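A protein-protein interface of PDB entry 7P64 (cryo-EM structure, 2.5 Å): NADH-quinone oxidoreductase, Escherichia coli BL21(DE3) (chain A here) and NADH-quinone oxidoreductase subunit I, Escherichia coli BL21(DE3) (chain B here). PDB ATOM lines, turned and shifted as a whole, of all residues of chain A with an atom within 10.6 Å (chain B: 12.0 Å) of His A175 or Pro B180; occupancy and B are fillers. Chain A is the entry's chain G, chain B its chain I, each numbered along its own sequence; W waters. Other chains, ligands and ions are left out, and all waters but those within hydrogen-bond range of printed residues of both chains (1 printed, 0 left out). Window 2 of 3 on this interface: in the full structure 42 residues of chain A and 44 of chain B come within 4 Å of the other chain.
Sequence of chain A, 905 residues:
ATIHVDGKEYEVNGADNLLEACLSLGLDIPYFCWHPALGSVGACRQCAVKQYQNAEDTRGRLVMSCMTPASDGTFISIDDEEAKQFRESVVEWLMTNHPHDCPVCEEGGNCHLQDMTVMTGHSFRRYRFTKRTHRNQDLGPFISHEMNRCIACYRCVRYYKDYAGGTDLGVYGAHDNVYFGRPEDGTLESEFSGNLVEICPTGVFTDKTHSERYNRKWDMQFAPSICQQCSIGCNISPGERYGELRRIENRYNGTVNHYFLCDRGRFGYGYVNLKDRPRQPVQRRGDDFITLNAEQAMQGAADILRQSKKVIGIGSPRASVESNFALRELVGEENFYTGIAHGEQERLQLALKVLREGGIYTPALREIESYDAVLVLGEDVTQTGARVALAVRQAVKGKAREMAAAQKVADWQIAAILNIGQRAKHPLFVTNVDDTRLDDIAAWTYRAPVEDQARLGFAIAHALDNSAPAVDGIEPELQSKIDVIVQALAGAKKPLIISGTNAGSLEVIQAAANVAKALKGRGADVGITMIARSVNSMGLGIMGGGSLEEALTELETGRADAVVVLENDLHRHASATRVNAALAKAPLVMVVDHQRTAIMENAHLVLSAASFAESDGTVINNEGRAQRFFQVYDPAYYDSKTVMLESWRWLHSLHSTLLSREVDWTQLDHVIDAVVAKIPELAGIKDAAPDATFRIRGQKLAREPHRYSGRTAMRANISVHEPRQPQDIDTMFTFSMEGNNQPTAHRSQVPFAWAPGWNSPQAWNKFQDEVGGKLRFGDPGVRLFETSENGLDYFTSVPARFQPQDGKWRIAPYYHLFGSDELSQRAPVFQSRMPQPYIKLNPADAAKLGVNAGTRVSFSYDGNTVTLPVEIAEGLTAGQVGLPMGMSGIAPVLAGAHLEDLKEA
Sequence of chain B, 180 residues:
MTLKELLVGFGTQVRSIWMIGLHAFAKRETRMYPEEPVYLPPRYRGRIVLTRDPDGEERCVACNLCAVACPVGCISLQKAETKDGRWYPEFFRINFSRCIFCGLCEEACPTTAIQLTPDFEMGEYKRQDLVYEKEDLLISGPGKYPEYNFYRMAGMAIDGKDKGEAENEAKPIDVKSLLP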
ATOM      1  N   ALA A  43      -0.623 -25.207 -11.790  1.00  0.00           N
ATOM      2  CA  ALA A  43      -0.986 -23.794 -11.803  1.00  0.00           C
ATOM      3  C   ALA A  43      -2.031 -23.452 -10.742  1.00  0.00           C
ATOM      4  O   ALA A  43      -1.788 -22.601  -9.886  1.00  0.00           O
ATOM      5  CB  ALA A  43      -1.484 -23.398 -13.196  1.00  0.00           C
ATOM      6  N   LEU A  94     -10.448 -18.099  -5.748  1.00  0.00           N
ATOM      7  CA  LEU A  94     -11.064 -18.084  -7.071  1.00  0.00           C
ATOM      8  C   LEU A  94     -12.433 -17.412  -7.052  1.00  0.00           C
ATOM      9  O   LEU A  94     -12.850 -16.838  -8.062  1.00  0.00           O
ATOM     10  CB  LEU A  94     -11.178 -19.504  -7.616  1.00  0.00           C
ATOM     11  CG  LEU A  94      -9.852 -20.176  -7.955  1.00  0.00           C
ATOM     12  CD1 LEU A  94     -10.090 -21.592  -8.417  1.00  0.00           C
ATOM     13  CD2 LEU A  94      -9.111 -19.382  -9.010  1.00  0.00           C
ATOM     14  N   ASN A  97     -13.215 -12.851  -7.377  1.00  0.00           N
ATOM     15  CA  ASN A  97     -13.484 -12.081  -8.580  1.00  0.00           C
ATOM     16  C   ASN A  97     -14.532 -12.714  -9.479  1.00  0.00           C
ATOM     17  O   ASN A  97     -14.802 -12.178 -10.558  1.00  0.00           O
ATOM     18  CB  ASN A  97     -12.189 -11.877  -9.367  1.00  0.00           C
ATOM     19  CG  ASN A  97     -11.197 -11.021  -8.624  1.00  0.00           C
ATOM     20  OD1 ASN A  97     -11.480  -9.875  -8.288  1.00  0.00           O
ATOM     21  ND2 ASN A  97     -10.027 -11.576  -8.353  1.00  0.00           N
ATOM     22  N   ARG A 132     -12.808  -7.853 -10.259  1.00  0.00           N
ATOM     23  CA  ARG A 132     -12.294  -7.446 -11.557  1.00  0.00           C
ATOM     24  C   ARG A 132     -13.227  -7.916 -12.666  1.00  0.00           C
ATOM     25  O   ARG A 132     -13.905  -8.939 -12.549  1.00  0.00           O
ATOM     26  CB  ARG A 132     -10.882  -7.991 -11.779  1.00  0.00           C
ATOM     27  CG  ARG A 132     -10.775  -9.502 -11.810  1.00  0.00           C
ATOM     28  CD  ARG A 132     -10.553 -10.019 -13.221  1.00  0.00           C
ATOM     29  NE  ARG A 132     -10.700 -11.466 -13.307  1.00  0.00           N
ATOM     30  CZ  ARG A 132     -11.860 -12.101 -13.417  1.00  0.00           C
ATOM     31  NH1 ARG A 132     -13.008 -11.449 -13.443  1.00  0.00           N
ATOM     32  NH2 ARG A 132     -11.865 -13.427 -13.501  1.00  0.00           N
ATOM     33  N   HIS A 134     -13.887  -7.963 -17.223  1.00  0.00           N
ATOM     34  CA  HIS A 134     -13.230  -8.040 -18.516  1.00  0.00           C
ATOM     35  C   HIS A 134     -14.244  -7.823 -19.624  1.00  0.00           C
ATOM     36  O   HIS A 134     -15.411  -8.197 -19.500  1.00  0.00           O
ATOM     37  CB  HIS A 134     -12.545  -9.394 -18.720  1.00  0.00           C
ATOM     38  CG  HIS A 134     -11.237  -9.524 -18.010  1.00  0.00           C
ATOM     39  ND1 HIS A 134     -10.164  -8.704 -18.277  1.00  0.00           N
ATOM     40  CD2 HIS A 134     -10.826 -10.385 -17.051  1.00  0.00           C
ATOM     41  CE1 HIS A 134      -9.149  -9.051 -17.508  1.00  0.00           C
ATOM     42  NE2 HIS A 134      -9.524 -10.068 -16.756  1.00  0.00           N
ATOM     43  N   MET A 147     -15.054 -13.635 -20.402  1.00  0.00           N
ATOM     44  CA  MET A 147     -13.819 -13.701 -19.632  1.00  0.00           C
ATOM     45  C   MET A 147     -13.985 -13.371 -18.157  1.00  0.00           C
ATOM     46  O   MET A 147     -13.027 -13.549 -17.402  1.00  0.00           O
ATOM     47  CB  MET A 147     -12.760 -12.771 -20.224  1.00  0.00           C
ATOM     48  CG  MET A 147     -11.738 -13.476 -21.087  1.00  0.00           C
ATOM     49  SD  MET A 147     -10.767 -14.683 -20.168  1.00  0.00           S
ATOM     50  CE  MET A 147     -10.001 -13.641 -18.936  1.00  0.00           C
ATOM     51  N   CYS A 150     -13.415 -16.491 -15.871  1.00  0.00           N
ATOM     52  CA  CYS A 150     -12.148 -17.202 -15.937  1.00  0.00           C
ATOM     53  C   CYS A 150     -11.496 -17.312 -14.568  1.00  0.00           C
ATOM     54  O   CYS A 150     -11.488 -16.362 -13.784  1.00  0.00           O
ATOM     55  CB  CYS A 150     -11.211 -16.504 -16.915  1.00  0.00           C
ATOM     56  SG  CYS A 150      -9.600 -17.257 -17.048  1.00  0.00           S
ATOM     57  N   ILE A 151     -10.948 -18.489 -14.284  1.00  0.00           N
ATOM     58  CA  ILE A 151     -10.206 -18.739 -13.059  1.00  0.00           C
ATOM     59  C   ILE A 151      -8.714 -18.882 -13.327  1.00  0.00           C
ATOM     60  O   ILE A 151      -7.965 -19.252 -12.421  1.00  0.00           O
ATOM     61  CB  ILE A 151     -10.749 -19.970 -12.318  1.00  0.00           C
ATOM     62  CG1 ILE A 151     -10.727 -21.184 -13.239  1.00  0.00           C
ATOM     63  CG2 ILE A 151     -12.152 -19.705 -11.803  1.00  0.00           C
ATOM     64  CD1 ILE A 151     -10.880 -22.477 -12.534  1.00  0.00           C
ATOM     65  N   ALA A 152      -8.275 -18.595 -14.558  1.00  0.00           N
ATOM     66  CA  ALA A 152      -6.865 -18.605 -14.968  1.00  0.00           C
ATOM     67  C   ALA A 152      -6.209 -19.960 -14.708  1.00  0.00           C
ATOM     68  O   ALA A 152      -5.150 -20.059 -14.089  1.00  0.00           O
ATOM     69  CB  ALA A 152      -6.079 -17.475 -14.300  1.00  0.00           C
ATOM     70  N   CYS A 153      -6.862 -21.013 -15.178  1.00  0.00           N
ATOM     71  CA  CYS A 153      -6.347 -22.361 -15.024  1.00  0.00           C
ATOM     72  C   CYS A 153      -5.469 -22.803 -16.187  1.00  0.00           C
ATOM     73  O   CYS A 153      -4.873 -23.881 -16.110  1.00  0.00           O
ATOM     74  CB  CYS A 153      -7.511 -23.335 -14.849  1.00  0.00           C
ATOM     75  SG  CYS A 153      -8.308 -23.809 -16.377  1.00  0.00           S
ATOM     76  N   TYR A 154      -5.401 -22.006 -17.257  1.00  0.00           N
ATOM     77  CA  TYR A 154      -4.521 -22.190 -18.413  1.00  0.00           C
ATOM     78  C   TYR A 154      -4.819 -23.461 -19.204  1.00  0.00           C
ATOM     79  O   TYR A 154      -3.977 -23.910 -19.978  1.00  0.00           O
ATOM     80  CB  TYR A 154      -3.040 -22.163 -18.010  1.00  0.00           C
ATOM     81  CG  TYR A 154      -2.570 -20.819 -17.515  1.00  0.00           C
ATOM     82  CD1 TYR A 154      -2.773 -20.438 -16.199  1.00  0.00           C
ATOM     83  CD2 TYR A 154      -1.926 -19.933 -18.362  1.00  0.00           C
ATOM     84  CE1 TYR A 154      -2.355 -19.215 -15.742  1.00  0.00           C
ATOM     85  CE2 TYR A 154      -1.502 -18.705 -17.912  1.00  0.00           C
ATOM     86  CZ  TYR A 154      -1.719 -18.352 -16.600  1.00  0.00           C
ATOM     87  OH  TYR A 154      -1.302 -17.131 -16.137  1.00  0.00           O
ATOM     88  N   VAL A 171      -2.636 -16.305 -23.984  1.00  0.00           N
ATOM     89  CA  VAL A 171      -2.808 -15.621 -22.711  1.00  0.00           C
ATOM     90  C   VAL A 171      -2.037 -14.310 -22.778  1.00  0.00           C
ATOM     91  O   VAL A 171      -0.888 -14.275 -23.235  1.00  0.00           O
ATOM     92  CB  VAL A 171      -2.358 -16.502 -21.529  1.00  0.00           C
ATOM     93  CG1 VAL A 171      -0.995 -17.129 -21.783  1.00  0.00           C
ATOM     94  CG2 VAL A 171      -2.374 -15.730 -20.224  1.00  0.00           C
ATOM     95  N   TYR A 172      -2.689 -13.229 -22.371  1.00  0.00           N
ATOM     96  CA  TYR A 172      -2.150 -11.886 -22.456  1.00  0.00           C
ATOM     97  C   TYR A 172      -2.239 -11.225 -21.095  1.00  0.00           C
ATOM     98  O   TYR A 172      -3.023 -11.626 -20.235  1.00  0.00           O
ATOM     99  CB  TYR A 172      -2.899 -11.047 -23.494  1.00  0.00           C
ATOM    100  CG  TYR A 172      -3.245 -11.849 -24.707  1.00  0.00           C
ATOM    101  CD1 TYR A 172      -2.270 -12.185 -25.631  1.00  0.00           C
ATOM    102  CD2 TYR A 172      -4.531 -12.315 -24.909  1.00  0.00           C
ATOM    103  CE1 TYR A 172      -2.569 -12.938 -26.731  1.00  0.00           C
ATOM    104  CE2 TYR A 172      -4.839 -13.068 -26.005  1.00  0.00           C
ATOM    105  CZ  TYR A 172      -3.856 -13.376 -26.912  1.00  0.00           C
ATOM    106  OH  TYR A 172      -4.156 -14.134 -28.009  1.00  0.00           O
ATOM    107  N   GLY A 173      -1.414 -10.211 -20.907  1.00  0.00           N
ATOM    108  CA  GLY A 173      -1.466  -9.458 -19.681  1.00  0.00           C
ATOM    109  C   GLY A 173      -0.595 -10.018 -18.585  1.00  0.00           C
ATOM    110  O   GLY A 173       0.451 -10.619 -18.837  1.00  0.00           O
ATOM    111  N   ALA A 174      -1.052  -9.846 -17.354  1.00  0.00           N
ATOM    112  CA  ALA A 174      -0.191  -9.905 -16.187  1.00  0.00           C
ATOM    113  C   ALA A 174      -0.967 -10.412 -14.984  1.00  0.00           C
ATOM    114  O   ALA A 174      -1.963 -11.124 -15.136  1.00  0.00           O
ATOM    115  CB  ALA A 174       0.427  -8.535 -15.907  1.00  0.00           C
ATOM    116  N   HIS A 175      -0.518 -10.009 -13.799  1.00  0.00           N
ATOM    117  CA  HIS A 175      -0.780 -10.564 -12.476  1.00  0.00           C
ATOM    118  C   HIS A 175      -2.177 -11.115 -12.221  1.00  0.00           C
ATOM    119  O   HIS A 175      -2.347 -12.328 -12.127  1.00  0.00           O
ATOM    120  CB  HIS A 175      -0.519  -9.436 -11.483  1.00  0.00           C
ATOM    121  CG  HIS A 175      -0.815  -8.080 -12.050  1.00  0.00           C
ATOM    122  ND1 HIS A 175      -2.075  -7.523 -12.027  1.00  0.00           N
ATOM    123  CD2 HIS A 175      -0.024  -7.186 -12.688  1.00  0.00           C
ATOM    124  CE1 HIS A 175      -2.045  -6.340 -12.613  1.00  0.00           C
ATOM    125  NE2 HIS A 175      -0.811  -6.111 -13.023  1.00  0.00           N
ATOM    126  N   ASP A 176      -3.190 -10.264 -12.175  1.00  0.00           N
ATOM    127  CA  ASP A 176      -4.562 -10.728 -12.073  1.00  0.00           C
ATOM    128  C   ASP A 176      -5.392 -10.242 -13.243  1.00  0.00           C
ATOM    129  O   ASP A 176      -6.605 -10.474 -13.270  1.00  0.00           O
ATOM    130  CB  ASP A 176      -5.198 -10.284 -10.747  1.00  0.00           C
ATOM    131  CG  ASP A 176      -5.117  -8.790 -10.529  1.00  0.00           C
ATOM    132  OD1 ASP A 176      -4.299  -8.126 -11.199  1.00  0.00           O
ATOM    133  OD2 ASP A 176      -5.877  -8.275  -9.683  1.00  0.00           O
ATOM    134  N   ASN A 177      -4.765  -9.572 -14.205  1.00  0.00           N
ATOM    135  CA  ASN A 177      -5.392  -9.168 -15.451  1.00  0.00           C
ATOM    136  C   ASN A 177      -5.055 -10.120 -16.593  1.00  0.00           C
ATOM    137  O   ASN A 177      -4.955  -9.690 -17.745  1.00  0.00           O
ATOM    138  CB  ASN A 177      -4.973  -7.744 -15.806  1.00  0.00           C
ATOM    139  CG  ASN A 177      -6.106  -6.930 -16.371  1.00  0.00           C
ATOM    140  OD1 ASN A 177      -7.256  -7.089 -15.972  1.00  0.00           O
ATOM    141  ND2 ASN A 177      -5.792  -6.055 -17.315  1.00  0.00           N
ATOM    142  N   VAL A 178      -4.852 -11.403 -16.289  1.00  0.00           N
ATOM    143  CA  VAL A 178      -4.590 -12.388 -17.330  1.00  0.00           C
ATOM    144  C   VAL A 178      -5.840 -12.575 -18.175  1.00  0.00           C
ATOM    145  O   VAL A 178      -6.930 -12.844 -17.656  1.00  0.00           O
ATOM    146  CB  VAL A 178      -4.132 -13.723 -16.721  1.00  0.00           C
ATOM    147  CG1 VAL A 178      -2.623 -13.837 -16.763  1.00  0.00           C
ATOM    148  CG2 VAL A 178      -4.646 -13.874 -15.302  1.00  0.00           C
ATOM    149  N   TYR A 179      -5.685 -12.430 -19.483  1.00  0.00           N
ATOM    150  CA  TYR A 179      -6.776 -12.517 -20.439  1.00  0.00           C
ATOM    151  C   TYR A 179      -6.517 -13.691 -21.367  1.00  0.00           C
ATOM    152  O   TYR A 179      -5.427 -13.814 -21.922  1.00  0.00           O
ATOM    153  CB  TYR A 179      -6.894 -11.219 -21.235  1.00  0.00           C
ATOM    154  CG  TYR A 179      -8.193 -11.051 -21.975  1.00  0.00           C
ATOM    155  CD1 TYR A 179      -8.348 -11.540 -23.263  1.00  0.00           C
ATOM    156  CD2 TYR A 179      -9.262 -10.388 -21.392  1.00  0.00           C
ATOM    157  CE1 TYR A 179      -9.530 -11.385 -23.942  1.00  0.00           C
ATOM    158  CE2 TYR A 179     -10.444 -10.227 -22.064  1.00  0.00           C
ATOM    159  CZ  TYR A 179     -10.574 -10.727 -23.339  1.00  0.00           C
ATOM    160  OH  TYR A 179     -11.754 -10.568 -24.016  1.00  0.00           O
ATOM    161  N   PHE A 180      -7.511 -14.547 -21.541  1.00  0.00           N
ATOM    162  CA  PHE A 180      -7.376 -15.719 -22.394  1.00  0.00           C
ATOM    163  C   PHE A 180      -8.277 -15.539 -23.605  1.00  0.00           C
ATOM    164  O   PHE A 180      -9.502 -15.486 -23.466  1.00  0.00           O
ATOM    165  CB  PHE A 180      -7.720 -16.993 -21.627  1.00  0.00           C
ATOM    166  CG  PHE A 180      -6.753 -17.312 -20.524  1.00  0.00           C
ATOM    167  CD1 PHE A 180      -6.895 -16.740 -19.272  1.00  0.00           C
ATOM    168  CD2 PHE A 180      -5.695 -18.173 -20.741  1.00  0.00           C
ATOM    169  CE1 PHE A 180      -6.007 -17.025 -18.263  1.00  0.00           C
ATOM    170  CE2 PHE A 180      -4.808 -18.466 -19.733  1.00  0.00           C
ATOM    171  CZ  PHE A 180      -4.961 -17.889 -18.495  1.00  0.00           C
ATOM    172  N   ALA B 170     -15.433  -3.659 -10.465  1.00  0.00           N
ATOM    173  CA  ALA B 170     -14.495  -2.659 -10.941  1.00  0.00           C
ATOM    174  C   ALA B 170     -14.580  -2.563 -12.457  1.00  0.00           C
ATOM    175  O   ALA B 170     -15.019  -3.494 -13.135  1.00  0.00           O
ATOM    176  CB  ALA B 170     -13.067  -2.998 -10.508  1.00  0.00           C
ATOM    177  N   LYS B 171     -14.173  -1.414 -12.982  1.00  0.00           N
ATOM    178  CA  LYS B 171     -14.154  -1.229 -14.423  1.00  0.00           C
ATOM    179  C   LYS B 171     -13.105  -2.146 -15.047  1.00  0.00           C
ATOM    180  O   LYS B 171     -12.053  -2.379 -14.446  1.00  0.00           O
ATOM    181  CB  LYS B 171     -13.856   0.227 -14.776  1.00  0.00           C
ATOM    182  CG  LYS B 171     -14.952   1.203 -14.380  1.00  0.00           C
ATOM    183  CD  LYS B 171     -16.309   0.769 -14.910  1.00  0.00           C
ATOM    184  CE  LYS B 171     -16.508   1.213 -16.351  1.00  0.00           C
ATOM    185  NZ  LYS B 171     -17.223   0.188 -17.159  1.00  0.00           N
ATOM    186  N   PRO B 172     -13.375  -2.707 -16.225  1.00  0.00           N
ATOM    187  CA  PRO B 172     -12.405  -3.614 -16.847  1.00  0.00           C
ATOM    188  C   PRO B 172     -11.133  -2.887 -17.253  1.00  0.00           C
ATOM    189  O   PRO B 172     -11.168  -1.761 -17.752  1.00  0.00           O
ATOM    190  CB  PRO B 172     -13.154  -4.156 -18.069  1.00  0.00           C
ATOM    191  CG  PRO B 172     -14.228  -3.173 -18.329  1.00  0.00           C
ATOM    192  CD  PRO B 172     -14.616  -2.606 -17.008  1.00  0.00           C
ATOM    193  N   ILE B 173     -10.004  -3.545 -17.019  1.00  0.00           N
ATOM    194  CA  ILE B 173      -8.688  -3.014 -17.346  1.00  0.00           C
ATOM    195  C   ILE B 173      -8.167  -3.786 -18.545  1.00  0.00           C
ATOM    196  O   ILE B 173      -8.040  -5.016 -18.493  1.00  0.00           O
ATOM    197  CB  ILE B 173      -7.720  -3.121 -16.158  1.00  0.00           C
ATOM    198  CG1 ILE B 173      -8.289  -2.397 -14.938  1.00  0.00           C
ATOM    199  CG2 ILE B 173      -6.365  -2.557 -16.526  1.00  0.00           C
ATOM    200  CD1 ILE B 173      -7.660  -2.818 -13.634  1.00  0.00           C
ATOM    201  N   ASP B 174      -7.879  -3.071 -19.626  1.00  0.00           N
ATOM    202  CA  ASP B 174      -7.333  -3.699 -20.817  1.00  0.00           C
ATOM    203  C   ASP B 174      -5.914  -4.182 -20.548  1.00  0.00           C
ATOM    204  O   ASP B 174      -5.172  -3.592 -19.759  1.00  0.00           O
ATOM    205  CB  ASP B 174      -7.347  -2.714 -21.987  1.00  0.00           C
ATOM    206  CG  ASP B 174      -7.285  -3.401 -23.341  1.00  0.00           C
ATOM    207  OD1 ASP B 174      -6.792  -4.543 -23.430  1.00  0.00           O
ATOM    208  OD2 ASP B 174      -7.735  -2.788 -24.331  1.00  0.00           O
ATOM    209  N   VAL B 175      -5.536  -5.273 -21.217  1.00  0.00           N
ATOM    210  CA  VAL B 175      -4.172  -5.772 -21.099  1.00  0.00           C
ATOM    211  C   VAL B 175      -3.179  -4.853 -21.795  1.00  0.00           C
ATOM    212  O   VAL B 175      -1.975  -4.932 -21.527  1.00  0.00           O
ATOM    213  CB  VAL B 175      -4.063  -7.205 -21.651  1.00  0.00           C
ATOM    214  CG1 VAL B 175      -4.809  -8.172 -20.755  1.00  0.00           C
ATOM    215  CG2 VAL B 175      -4.591  -7.273 -23.074  1.00  0.00           C
ATOM    216  N   LYS B 176      -3.650  -3.975 -22.676  1.00  0.00           N
ATOM    217  CA  LYS B 176      -2.803  -3.007 -23.355  1.00  0.00           C
ATOM    218  C   LYS B 176      -2.584  -1.737 -22.546  1.00  0.00           C
ATOM    219  O   LYS B 176      -1.890  -0.835 -23.023  1.00  0.00           O
ATOM    220  CB  LYS B 176      -3.406  -2.645 -24.713  1.00  0.00           C
ATOM    221  CG  LYS B 176      -3.667  -3.833 -25.613  1.00  0.00           C
ATOM    222  CD  LYS B 176      -3.968  -3.382 -27.027  1.00  0.00           C
ATOM    223  CE  LYS B 176      -5.396  -3.700 -27.416  1.00  0.00           C
ATOM    224  NZ  LYS B 176      -6.061  -2.543 -28.079  1.00  0.00           N
ATOM    225  N   SER B 177      -3.157  -1.643 -21.349  1.00  0.00           N
ATOM    226  CA  SER B 177      -3.024  -0.445 -20.532  1.00  0.00           C
ATOM    227  C   SER B 177      -1.590  -0.270 -20.045  1.00  0.00           C
ATOM    228  O   SER B 177      -0.867  -1.238 -19.800  1.00  0.00           O
ATOM    229  CB  SER B 177      -3.975  -0.506 -19.339  1.00  0.00           C
ATOM    230  OG  SER B 177      -3.561  -1.490 -18.410  1.00  0.00           O
ATOM    231  N   LEU B 178      -1.185   0.992 -19.904  1.00  0.00           N
ATOM    232  CA  LEU B 178       0.199   1.325 -19.593  1.00  0.00           C
ATOM    233  C   LEU B 178       0.560   1.104 -18.132  1.00  0.00           C
ATOM    234  O   LEU B 178       1.751   1.045 -17.811  1.00  0.00           O
ATOM    235  CB  LEU B 178       0.475   2.780 -19.967  1.00  0.00           C
ATOM    236  CG  LEU B 178       0.007   3.193 -21.359  1.00  0.00           C
ATOM    237  CD1 LEU B 178       0.030   4.701 -21.503  1.00  0.00           C
ATOM    238  CD2 LEU B 178       0.871   2.537 -22.417  1.00  0.00           C
ATOM    239  N   LEU B 179      -0.424   0.992 -17.250  1.00  0.00           N
ATOM    240  CA  LEU B 179      -0.134   0.849 -15.832  1.00  0.00           C
ATOM    241  C   LEU B 179       0.423  -0.542 -15.539  1.00  0.00           C
ATOM    242  O   LEU B 179      -0.093  -1.539 -16.053  1.00  0.00           O
ATOM    243  CB  LEU B 179      -1.392   1.096 -15.004  1.00  0.00           C
ATOM    244  CG  LEU B 179      -1.769   2.563 -14.808  1.00  0.00           C
ATOM    245  CD1 LEU B 179      -3.016   2.687 -13.953  1.00  0.00           C
ATOM    246  CD2 LEU B 179      -0.613   3.321 -14.183  1.00  0.00           C
ATOM    247  N   PRO B 180       1.480  -0.644 -14.719  1.00  0.00           N
ATOM    248  CA  PRO B 180       2.120  -1.921 -14.381  1.00  0.00           C
ATOM    249  C   PRO B 180       1.209  -2.851 -13.585  1.00  0.00           C
ATOM    250  O   PRO B 180       0.292  -2.367 -12.919  1.00  0.00           O
ATOM    251  CB  PRO B 180       3.327  -1.498 -13.535  1.00  0.00           C
ATOM    252  CG  PRO B 180       3.519  -0.048 -13.813  1.00  0.00           C
ATOM    253  CD  PRO B 180       2.158   0.491 -14.073  1.00  0.00           C
HETATM  254  O   HOH W   1      -9.701  -6.103 -15.738  1.00  0.00           O
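ND2 of Asn A177 lies within hydrogen-bond range of O of Ile B173, 2.7 Å away.
The backbone NH (N) of Tyr A172 is in hydrogen-bond range of the backbone carbonyl oxygen (O) of Tyr A179 (2.8 Å).
OD1 of Asp A176 is in hydrogen-bond range of ND1 of His A175.
N of Lys B176 lies close to OD1 of Asp B174, at 3.3 Å.
OG of Ser B177 lies within hydrogen-bond range of O of Asp B174 (3.0 Å).
Among the printed residues, pairs that only touch across the chains: His A134 with Pro B172, Tyr A172 with Val B175, Gly A173 with Val B175, His A175 with Pro B180, Asn A177 with Asp B174, Asn A177 with Val B175 and Tyr A179 with Val B175.
Asn A97 touches none of the printed residues of chain B.
Printed residues of chain B within 4 Å of His A134: Pro B172.
Of the printed residues of chain B, Tyr A172 touches Val B175 (3.9 Å).
His A175 touches just one residue of chain B: Pro B180 (3.9 Å).
No residue of chain B comes within 4 Å of Asp A176.
Of chain B, only Ile B173 (2.7 Å), Asp B174 (3.5 Å) and Val B175 (3.4 Å) come within 4 Å of Asn A177.
No residue of chain B comes within 4 Å of Val A178.
Printed residues of chain B within 4 Å of Tyr A179: Val B175 (3.7 Å).
Printed residues of chain A within 4 Å of Asp B174: Asn A177 (3.5 Å).
Of the printed residues of chain A, Val B175 touches Tyr A172, Gly A173, Asn A177 and Tyr A179.
No residue of chain A comes within 4 Å of Leu B179.
Pro B180 touches just one residue of chain A: His A175.
The nearest residue of chain A that does not touch Pro B180 is Ala A174 (6.2 Å).
The nearest printed residue of chain B that does not touch Tyr A179 is Ile B173 (6.2 Å).
Of the 11 printed residues of chain B, 5 touch a printed residue of chain A.
Printed residues of chain B that touch a printed residue of chain A: Pro B172, Ile B173, Asp B174, Val B175 and Pro B180.
Hydrophobic or aromatic side chains of chain B within 4 Å of the printed part of chain A: Pro B172, Ile B173 and Val B175.
Printed residues of chain A that touch a printed residue of chain B: His A134, Tyr A172, Gly A173, His A175, Asn A177 and Tyr A179.
Hydrophobic or aromatic side chains of chain A that line the printed part of chain B: His A175 and Tyr A179.
Among the printed residues, 8 pairs touch across the chains.
Among the printed residues, no Asp or Glu carboxylate lies within 4 Å of a Lys or Arg side-chain nitrogen of the other chain.
Water W1 lies within hydrogen-bond range of the side-chain amide oxygen of Asn A177 (2.6 Å) and the backbone NH of Ile B173 (2.9 Å).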
